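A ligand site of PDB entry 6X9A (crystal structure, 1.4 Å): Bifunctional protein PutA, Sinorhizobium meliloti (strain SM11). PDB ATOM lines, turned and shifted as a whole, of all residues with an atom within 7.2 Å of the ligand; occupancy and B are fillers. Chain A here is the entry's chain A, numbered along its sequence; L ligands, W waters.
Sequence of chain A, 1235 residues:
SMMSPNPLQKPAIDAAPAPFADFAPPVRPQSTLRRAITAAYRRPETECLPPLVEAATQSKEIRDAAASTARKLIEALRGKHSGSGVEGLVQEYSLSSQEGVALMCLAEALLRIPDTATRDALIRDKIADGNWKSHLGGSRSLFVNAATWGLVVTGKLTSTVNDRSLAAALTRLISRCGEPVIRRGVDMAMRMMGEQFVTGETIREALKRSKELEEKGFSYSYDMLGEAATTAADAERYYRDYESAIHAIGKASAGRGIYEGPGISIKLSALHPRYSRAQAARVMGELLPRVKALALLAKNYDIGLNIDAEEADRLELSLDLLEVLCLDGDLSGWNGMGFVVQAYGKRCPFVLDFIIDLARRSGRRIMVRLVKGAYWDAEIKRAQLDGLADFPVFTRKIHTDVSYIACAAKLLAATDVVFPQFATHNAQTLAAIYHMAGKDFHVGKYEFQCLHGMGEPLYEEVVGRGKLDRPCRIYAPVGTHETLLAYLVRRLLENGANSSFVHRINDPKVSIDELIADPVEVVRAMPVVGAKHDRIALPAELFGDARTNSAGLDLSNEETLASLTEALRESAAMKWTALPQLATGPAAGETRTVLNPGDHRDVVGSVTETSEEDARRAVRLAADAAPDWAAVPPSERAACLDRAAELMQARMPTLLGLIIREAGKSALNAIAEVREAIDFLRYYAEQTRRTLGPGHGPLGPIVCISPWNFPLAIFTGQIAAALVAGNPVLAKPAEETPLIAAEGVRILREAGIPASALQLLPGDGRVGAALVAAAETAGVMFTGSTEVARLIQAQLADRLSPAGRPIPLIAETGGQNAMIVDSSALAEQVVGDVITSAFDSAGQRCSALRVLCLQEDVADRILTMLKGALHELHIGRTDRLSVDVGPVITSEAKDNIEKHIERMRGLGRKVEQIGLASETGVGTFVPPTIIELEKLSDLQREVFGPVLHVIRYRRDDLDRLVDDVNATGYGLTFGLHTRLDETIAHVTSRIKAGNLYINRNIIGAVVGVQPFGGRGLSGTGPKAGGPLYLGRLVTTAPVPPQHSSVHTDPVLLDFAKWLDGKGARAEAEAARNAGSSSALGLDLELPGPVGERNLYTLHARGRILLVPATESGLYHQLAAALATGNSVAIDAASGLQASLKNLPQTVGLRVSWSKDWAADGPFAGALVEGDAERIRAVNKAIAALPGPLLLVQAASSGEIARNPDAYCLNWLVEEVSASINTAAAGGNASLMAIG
Water W2 lies within hydrogen-bond range of an oxygen (O1) of the ligand (2.7 Å), the backbone NH of Cys 846 (3.0 Å) and the backbone NH of Ser 847 (3.2 Å). Water W1 lies within hydrogen-bond range of OH of Tyr 997 (2.7 Å), O of Ile 1002 (2.8 Å) and O2 of the ligand (2.9 Å). Water W3 lies within hydrogen-bond range of the backbone carbonyl oxygen of Ala 1005 (2.9 Å) and an oxygen (O3) of the ligand (3.1 Å).
O of Ser 847 lies within hydrogen-bond range of OG1 of Thr 973, 2.9 Å away. The backbone NH (N) of Phe 1012 lies within hydrogen-bond range of the backbone carbonyl oxygen (O) of Ala 1024 (2.9 Å). NE of Arg 845 lies within salt-bridge range of OD1 of Asp 840 (2.8 Å).
An oxygen (O1) of the ligand lies within salt-bridge range of the guanidinium group of Arg 845 (3.0 Å). The backbone NH (N) of Gly 1004 sits at hydrogen-bond distance from an oxygen (O2) of the ligand, 3.0 Å away. A nitrogen (N1) of the ligand lies within salt-bridge range of the side-chain carboxylate (OE1) of Glu 676 (2.8 Å). OG of Ser 847 sits at hydrogen-bond distance from O1 of the ligand (3.0 Å). The backbone NH of Ala 1005 sits at hydrogen-bond distance from an oxygen (O2) of the ligand (2.9 Å).
CZ of Phe 710 touches N1 of the ligand, 3.5 Å away. CD1 of Ile 714 touches C3 of the ligand (3.98 Å). Ile 1003 touches the ligand (C to O2, 3.8 Å). Phe 1012 touches the ligand. Hydrophobic or aromatic side chains that line the ligand: Phe 710, Ile 714, Ala 1005 and Phe 1012. Within 4 Å of the ligand: Glu 676, Phe 710, Ile 714, Arg 845, Ser 847, Ile 1003, Gly 1004, Ala 1005 and Phe 1012. The nearest printed residue that does not touch the ligand is Phe 680 (4.1 Å).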
ATOM      1  N   LYS A 665       1.852  13.955  -8.190  1.00  0.00           N
ATOM      2  CA  LYS A 665       3.025  13.153  -8.506  1.00  0.00           C
ATOM      3  C   LYS A 665       2.942  12.547  -9.897  1.00  0.00           C
ATOM      4  O   LYS A 665       1.864  12.354 -10.468  1.00  0.00           O
ATOM      5  CB  LYS A 665       3.165  12.018  -7.496  1.00  0.00           C
ATOM      6  CG  LYS A 665       3.333  12.505  -6.079  1.00  0.00           C
ATOM      7  CD  LYS A 665       4.176  11.506  -5.278  1.00  0.00           C
ATOM      8  CE  LYS A 665       4.526  12.059  -3.912  1.00  0.00           C
ATOM      9  NZ  LYS A 665       5.432  11.092  -3.204  1.00  0.00           N
ATOM     10  N   ALA A 672       6.497   4.067  -6.968  1.00  0.00           N
ATOM     11  CA  ALA A 672       7.501   3.903  -5.933  1.00  0.00           C
ATOM     12  C   ALA A 672       6.919   4.190  -4.564  1.00  0.00           C
ATOM     13  O   ALA A 672       7.300   3.553  -3.574  1.00  0.00           O
ATOM     14  CB  ALA A 672       8.704   4.797  -6.237  1.00  0.00           C
ATOM     15  N   GLU A 673       5.970   5.121  -4.479  1.00  0.00           N
ATOM     16  CA  GLU A 673       5.346   5.430  -3.195  1.00  0.00           C
ATOM     17  C   GLU A 673       4.466   4.284  -2.704  1.00  0.00           C
ATOM     18  O   GLU A 673       4.518   3.921  -1.521  1.00  0.00           O
ATOM     19  CB  GLU A 673       4.546   6.713  -3.263  1.00  0.00           C
ATOM     20  CG  GLU A 673       3.731   6.871  -1.977  1.00  0.00           C
ATOM     21  CD  GLU A 673       3.545   8.297  -1.558  1.00  0.00           C
ATOM     22  OE1 GLU A 673       3.281   8.531  -0.364  1.00  0.00           O
ATOM     23  OE2 GLU A 673       3.610   9.180  -2.438  1.00  0.00           O
ATOM     24  N   GLU A 676       6.667   1.667  -1.458  1.00  0.00           N
ATOM     25  CA  GLU A 676       7.212   1.977  -0.137  1.00  0.00           C
ATOM     26  C   GLU A 676       6.189   1.688   0.951  1.00  0.00           C
ATOM     27  O   GLU A 676       6.534   1.160   2.016  1.00  0.00           O
ATOM     28  CB  GLU A 676       7.653   3.445  -0.078  1.00  0.00           C
ATOM     29  CG  GLU A 676       8.400   3.830   1.189  1.00  0.00           C
ATOM     30  CD  GLU A 676       8.883   5.278   1.165  1.00  0.00           C
ATOM     31  OE1 GLU A 676       9.532   5.668   0.186  1.00  0.00           O
ATOM     32  OE2 GLU A 676       8.574   6.031   2.108  1.00  0.00           O
ATOM     33  N   PHE A 680       6.825  -0.935   3.940  1.00  0.00           N
ATOM     34  CA  PHE A 680       6.691  -0.635   5.363  1.00  0.00           C
ATOM     35  C   PHE A 680       5.808  -1.658   6.060  1.00  0.00           C
ATOM     36  O   PHE A 680       6.147  -2.156   7.136  1.00  0.00           O
ATOM     37  CB  PHE A 680       6.076   0.745   5.567  1.00  0.00           C
ATOM     38  CG  PHE A 680       7.052   1.896   5.515  1.00  0.00           C
ATOM     39  CD1 PHE A 680       8.228   1.879   6.240  1.00  0.00           C
ATOM     40  CD2 PHE A 680       6.760   3.016   4.745  1.00  0.00           C
ATOM     41  CE1 PHE A 680       9.099   2.955   6.194  1.00  0.00           C
ATOM     42  CE2 PHE A 680       7.630   4.103   4.686  1.00  0.00           C
ATOM     43  CZ  PHE A 680       8.801   4.085   5.402  1.00  0.00           C
ATOM     44  N   ASN A 709       4.013  15.282   1.169  1.00  0.00           N
ATOM     45  CA  ASN A 709       4.942  14.883   0.114  1.00  0.00           C
ATOM     46  C   ASN A 709       5.044  13.370  -0.036  1.00  0.00           C
ATOM     47  O   ASN A 709       5.426  12.893  -1.106  1.00  0.00           O
ATOM     48  CB  ASN A 709       6.317  15.514   0.332  1.00  0.00           C
ATOM     49  CG  ASN A 709       7.055  14.972   1.524  1.00  0.00           C
ATOM     50  OD1 ASN A 709       6.466  14.384   2.441  1.00  0.00           O
ATOM     51  ND2 ASN A 709       8.371  15.184   1.552  1.00  0.00           N
ATOM     52  N   PHE A 710       4.698  12.600   1.000  1.00  0.00           N
ATOM     53  CA  PHE A 710       4.579  11.145   0.906  1.00  0.00           C
ATOM     54  C   PHE A 710       3.276  10.764   1.588  1.00  0.00           C
ATOM     55  O   PHE A 710       3.266  10.158   2.672  1.00  0.00           O
ATOM     56  CB  PHE A 710       5.791  10.410   1.457  1.00  0.00           C
ATOM     57  CG  PHE A 710       6.969  10.510   0.543  1.00  0.00           C
ATOM     58  CD1 PHE A 710       7.103   9.620  -0.517  1.00  0.00           C
ATOM     59  CD2 PHE A 710       7.891  11.516   0.692  1.00  0.00           C
ATOM     60  CE1 PHE A 710       8.163   9.723  -1.393  1.00  0.00           C
ATOM     61  CE2 PHE A 710       8.971  11.628  -0.186  1.00  0.00           C
ATOM     62  CZ  PHE A 710       9.095  10.732  -1.227  1.00  0.00           C
ATOM     63  N   ALA A 713       2.926   6.729   1.684  1.00  0.00           N
ATOM     64  CA  ALA A 713       4.007   5.899   2.226  1.00  0.00           C
ATOM     65  C   ALA A 713       4.325   6.239   3.671  1.00  0.00           C
ATOM     66  O   ALA A 713       4.371   5.358   4.542  1.00  0.00           O
ATOM     67  CB  ALA A 713       5.259   5.982   1.353  1.00  0.00           C
ATOM     68  N   ILE A 714       4.575   7.515   3.964  1.00  0.00           N
ATOM     69  CA  ILE A 714       4.947   7.882   5.335  1.00  0.00           C
ATOM     70  C   ILE A 714       3.720   7.839   6.234  1.00  0.00           C
ATOM     71  O   ILE A 714       3.807   7.448   7.411  1.00  0.00           O
ATOM     72  CB  ILE A 714       5.683   9.233   5.350  1.00  0.00           C
ATOM     73  CG1 ILE A 714       7.077   9.030   4.735  1.00  0.00           C
ATOM     74  CG2 ILE A 714       5.774   9.785   6.792  1.00  0.00           C
ATOM     75  CD1 ILE A 714       7.928  10.293   4.670  1.00  0.00           C
ATOM     76  N   ASP A 840      13.227  15.495  -9.271  1.00  0.00           N
ATOM     77  CA  ASP A 840      12.189  14.496  -9.135  1.00  0.00           C
ATOM     78  C   ASP A 840      11.201  14.957  -8.067  1.00  0.00           C
ATOM     79  O   ASP A 840      11.611  15.528  -7.051  1.00  0.00           O
ATOM     80  CB  ASP A 840      12.852  13.175  -8.726  1.00  0.00           C
ATOM     81  CG  ASP A 840      11.890  12.049  -8.509  1.00  0.00           C
ATOM     82  OD1 ASP A 840      11.244  12.020  -7.438  1.00  0.00           O
ATOM     83  OD2 ASP A 840      11.806  11.177  -9.402  1.00  0.00           O
ATOM     84  N   ARG A 845      10.905  16.062  -2.117  1.00  0.00           N
ATOM     85  CA  ARG A 845      11.360  14.999  -1.242  1.00  0.00           C
ATOM     86  C   ARG A 845      12.206  15.608  -0.135  1.00  0.00           C
ATOM     87  O   ARG A 845      12.982  16.543  -0.371  1.00  0.00           O
ATOM     88  CB  ARG A 845      12.230  14.014  -2.018  1.00  0.00           C
ATOM     89  CG  ARG A 845      11.504  13.189  -3.056  1.00  0.00           C
ATOM     90  CD  ARG A 845      12.503  12.257  -3.705  1.00  0.00           C
ATOM     91  NE  ARG A 845      11.927  11.507  -4.814  1.00  0.00           N
ATOM     92  CZ  ARG A 845      11.462  10.265  -4.706  1.00  0.00           C
ATOM     93  NH1 ARG A 845      11.534   9.621  -3.547  1.00  0.00           N
ATOM     94  NH2 ARG A 845      10.950   9.668  -5.773  1.00  0.00           N
ATOM     95  N   CYS A 846      12.089  15.047   1.067  1.00  0.00           N
ATOM     96  CA  CYS A 846      12.988  15.466   2.126  1.00  0.00           C
ATOM     97  C   CYS A 846      14.424  15.106   1.786  1.00  0.00           C
ATOM     98  O   CYS A 846      15.359  15.791   2.231  1.00  0.00           O
ATOM     99  CB  CYS A 846      12.570  14.860   3.464  1.00  0.00           C
ATOM    100  SG  CYS A 846      11.006  15.527   4.045  1.00  0.00           S
ATOM    101  N   SER A 847      14.604  14.039   1.013  1.00  0.00           N
ATOM    102  CA  SER A 847      15.907  13.558   0.572  1.00  0.00           C
ATOM    103  C   SER A 847      16.475  14.342  -0.603  1.00  0.00           C
ATOM    104  O   SER A 847      17.599  14.035  -1.020  1.00  0.00           O
ATOM    105  CB  SER A 847      15.795  12.086   0.179  1.00  0.00           C
ATOM    106  OG  SER A 847      14.757  11.906  -0.775  1.00  0.00           O
ATOM    107  N   ALA A 848      15.755  15.326  -1.144  1.00  0.00           N
ATOM    108  CA  ALA A 848      16.166  15.923  -2.404  1.00  0.00           C
ATOM    109  C   ALA A 848      17.516  16.629  -2.303  1.00  0.00           C
ATOM    110  O   ALA A 848      17.898  17.155  -1.263  1.00  0.00           O
ATOM    111  CB  ALA A 848      15.109  16.930  -2.872  1.00  0.00           C
ATOM    112  N   THR A 973      20.261  13.283   3.913  1.00  0.00           N
ATOM    113  CA  THR A 973      20.913  12.547   2.838  1.00  0.00           C
ATOM    114  C   THR A 973      22.167  13.270   2.366  1.00  0.00           C
ATOM    115  O   THR A 973      22.318  14.485   2.516  1.00  0.00           O
ATOM    116  CB  THR A 973      19.979  12.297   1.653  1.00  0.00           C
ATOM    117  OG1 THR A 973      19.560  13.545   1.081  1.00  0.00           O
ATOM    118  CG2 THR A 973      18.762  11.454   2.063  1.00  0.00           C
ATOM    119  N   ASN A 995      21.932   9.099   5.766  1.00  0.00           N
ATOM    120  CA  ASN A 995      21.742   8.296   4.559  1.00  0.00           C
ATOM    121  C   ASN A 995      22.774   8.746   3.534  1.00  0.00           C
ATOM    122  O   ASN A 995      22.644   9.810   2.922  1.00  0.00           O
ATOM    123  CB  ASN A 995      20.315   8.415   4.008  1.00  0.00           C
ATOM    124  CG  ASN A 995      19.345   7.495   4.742  1.00  0.00           C
ATOM    125  OD1 ASN A 995      18.796   7.864   5.781  1.00  0.00           O
ATOM    126  ND2 ASN A 995      19.162   6.284   4.230  1.00  0.00           N
ATOM    127  N   TYR A 997      25.097   8.047   0.027  1.00  0.00           N
ATOM    128  CA  TYR A 997      24.951   7.431  -1.275  1.00  0.00           C
ATOM    129  C   TYR A 997      26.210   7.695  -2.076  1.00  0.00           C
ATOM    130  O   TYR A 997      26.601   8.857  -2.232  1.00  0.00           O
ATOM    131  CB  TYR A 997      23.735   8.005  -2.010  1.00  0.00           C
ATOM    132  CG  TYR A 997      22.425   7.729  -1.307  1.00  0.00           C
ATOM    133  CD1 TYR A 997      21.769   6.507  -1.476  1.00  0.00           C
ATOM    134  CD2 TYR A 997      21.856   8.665  -0.448  1.00  0.00           C
ATOM    135  CE1 TYR A 997      20.564   6.245  -0.839  1.00  0.00           C
ATOM    136  CE2 TYR A 997      20.657   8.415   0.207  1.00  0.00           C
ATOM    137  CZ  TYR A 997      20.022   7.205  -0.001  1.00  0.00           C
ATOM    138  OH  TYR A 997      18.828   6.925   0.643  1.00  0.00           O
ATOM    139  N   ILE A1002      20.543  10.276  -4.604  1.00  0.00           N
ATOM    140  CA  ILE A1002      20.389  10.339  -3.141  1.00  0.00           C
ATOM    141  C   ILE A1002      18.928  10.206  -2.712  1.00  0.00           C
ATOM    142  O   ILE A1002      18.604  10.494  -1.551  1.00  0.00           O
ATOM    143  CB  ILE A1002      21.074  11.569  -2.515  1.00  0.00           C
ATOM    144  CG1 ILE A1002      20.318  12.870  -2.863  1.00  0.00           C
ATOM    145  CG2 ILE A1002      22.550  11.664  -2.947  1.00  0.00           C
ATOM    146  CD1 ILE A1002      20.891  14.104  -2.169  1.00  0.00           C
ATOM    147  N   ILE A1003      18.056   9.731  -3.601  1.00  0.00           N
ATOM    148  CA  ILE A1003      16.618   9.718  -3.338  1.00  0.00           C
ATOM    149  C   ILE A1003      16.085   8.289  -3.393  1.00  0.00           C
ATOM    150  O   ILE A1003      16.752   7.358  -3.827  1.00  0.00           O
ATOM    151  CB  ILE A1003      15.832  10.644  -4.292  1.00  0.00           C
ATOM    152  CG1 ILE A1003      16.011  10.224  -5.746  1.00  0.00           C
ATOM    153  CG2 ILE A1003      16.251  12.112  -4.077  1.00  0.00           C
ATOM    154  CD1 ILE A1003      14.941  10.820  -6.706  1.00  0.00           C
ATOM    155  N   GLY A1004      14.847   8.125  -2.943  1.00  0.00           N
ATOM    156  CA  GLY A1004      14.202   6.826  -3.036  1.00  0.00           C
ATOM    157  C   GLY A1004      14.762   5.758  -2.107  1.00  0.00           C
ATOM    158  O   GLY A1004      14.890   4.599  -2.511  1.00  0.00           O
ATOM    159  N   ALA A1005      15.083   6.136  -0.860  1.00  0.00           N
ATOM    160  CA  ALA A1005      15.524   5.146   0.117  1.00  0.00           C
ATOM    161  C   ALA A1005      14.520   4.002   0.209  1.00  0.00           C
ATOM    162  O   ALA A1005      13.299   4.225   0.226  1.00  0.00           O
ATOM    163  CB  ALA A1005      15.651   5.814   1.481  1.00  0.00           C
ATOM    164  N   VAL A1006      15.052   2.786   0.253  1.00  0.00           N
ATOM    165  CA  VAL A1006      14.251   1.562   0.209  1.00  0.00           C
ATOM    166  C   VAL A1006      14.137   0.976   1.604  1.00  0.00           C
ATOM    167  O   VAL A1006      15.146   0.745   2.267  1.00  0.00           O
ATOM    168  CB  VAL A1006      14.877   0.549  -0.767  1.00  0.00           C
ATOM    169  CG1 VAL A1006      14.179  -0.807  -0.673  1.00  0.00           C
ATOM    170  CG2 VAL A1006      14.840   1.097  -2.180  1.00  0.00           C
ATOM    171  N   VAL A1007      12.901   0.718   2.033  1.00  0.00           N
ATOM    172  CA  VAL A1007      12.638   0.143   3.353  1.00  0.00           C
ATOM    173  C   VAL A1007      13.469  -1.107   3.562  1.00  0.00           C
ATOM    174  O   VAL A1007      13.493  -2.003   2.713  1.00  0.00           O
ATOM    175  CB  VAL A1007      11.138  -0.175   3.457  1.00  0.00           C
ATOM    176  CG1 VAL A1007      10.850  -0.920   4.760  1.00  0.00           C
ATOM    177  CG2 VAL A1007      10.324   1.112   3.408  1.00  0.00           C
ATOM    178  N   GLN A1010      17.933   0.751   2.667  1.00  0.00           N
ATOM    179  CA  GLN A1010      18.484   1.998   3.206  1.00  0.00           C
ATOM    180  C   GLN A1010      17.494   2.526   4.240  1.00  0.00           C
ATOM    181  O   GLN A1010      16.690   3.415   3.945  1.00  0.00           O
ATOM    182  CB  GLN A1010      18.748   3.052   2.126  1.00  0.00           C
ATOM    183  CG  GLN A1010      19.654   2.617   0.997  1.00  0.00           C
ATOM    184  CD  GLN A1010      18.882   2.143  -0.215  1.00  0.00           C
ATOM    185  OE1 GLN A1010      17.758   2.587  -0.474  1.00  0.00           O
ATOM    186  NE2 GLN A1010      19.469   1.215  -0.967  1.00  0.00           N
ATOM    187  N   PHE A1012      15.799   4.791   6.663  1.00  0.00           N
ATOM    188  CA  PHE A1012      15.794   6.209   6.330  1.00  0.00           C
ATOM    189  C   PHE A1012      15.648   7.080   7.567  1.00  0.00           C
ATOM    190  O   PHE A1012      14.720   6.906   8.362  1.00  0.00           O
ATOM    191  CB  PHE A1012      14.673   6.558   5.360  1.00  0.00           C
ATOM    192  CG  PHE A1012      14.771   7.964   4.869  1.00  0.00           C
ATOM    193  CD1 PHE A1012      15.749   8.318   3.965  1.00  0.00           C
ATOM    194  CD2 PHE A1012      13.886   8.946   5.321  1.00  0.00           C
ATOM    195  CE1 PHE A1012      15.872   9.624   3.500  1.00  0.00           C
ATOM    196  CE2 PHE A1012      14.001  10.248   4.861  1.00  0.00           C
ATOM    197  CZ  PHE A1012      14.984  10.584   3.934  1.00  0.00           C
ATOM    198  N   GLY A1013      16.554   8.038   7.698  1.00  0.00           N
ATOM    199  CA  GLY A1013      16.423   9.027   8.752  1.00  0.00           C
ATOM    200  C   GLY A1013      17.765   9.625   9.090  1.00  0.00           C
ATOM    201  O   GLY A1013      18.800   8.967   8.989  1.00  0.00           O
ATOM    202  N   ALA A1024      13.094   5.182  10.222  1.00  0.00           N
ATOM    203  CA  ALA A1024      11.990   4.440   9.630  1.00  0.00           C
ATOM    204  C   ALA A1024      12.550   3.364   8.706  1.00  0.00           C
ATOM    205  O   ALA A1024      13.623   3.515   8.122  1.00  0.00           O
ATOM    206  CB  ALA A1024      11.092   5.395   8.834  1.00  0.00           C
HETATM  207  C1  LIG L   1      12.406   8.248   2.221  1.00  0.00           C
HETATM  208  C2  LIG L   1      11.028   8.404   2.846  1.00  0.00           C
HETATM  209  C3  LIG L   1      10.133   8.870   1.680  1.00  0.00           C
HETATM  210  C4  LIG L   1      12.183   8.038   0.719  1.00  0.00           C
HETATM  211  C5  LIG L   1      13.045   9.052  -0.108  1.00  0.00           C
HETATM  212  N1  LIG L   1      10.702   8.186   0.482  1.00  0.00           N
HETATM  213  O1  LIG L   1      12.444  10.000  -0.669  1.00  0.00           O
HETATM  214  O2  LIG L   1      14.280   8.857  -0.126  1.00  0.00           O
HETATM  215  O3  LIG L   1      10.573   7.132   3.249  1.00  0.00           O
HETATM  216  O   HOH W   1      17.140   8.981   0.233  1.00  0.00           O
HETATM  217  O   HOH W   2      12.158  12.049   1.096  1.00  0.00           O
HETATM  218  O   HOH W   3      12.184   4.569   2.843  1.00  0.00           O
HETATM  219  O   HOH W   4      10.400   7.120   5.998  1.00  0.00           O
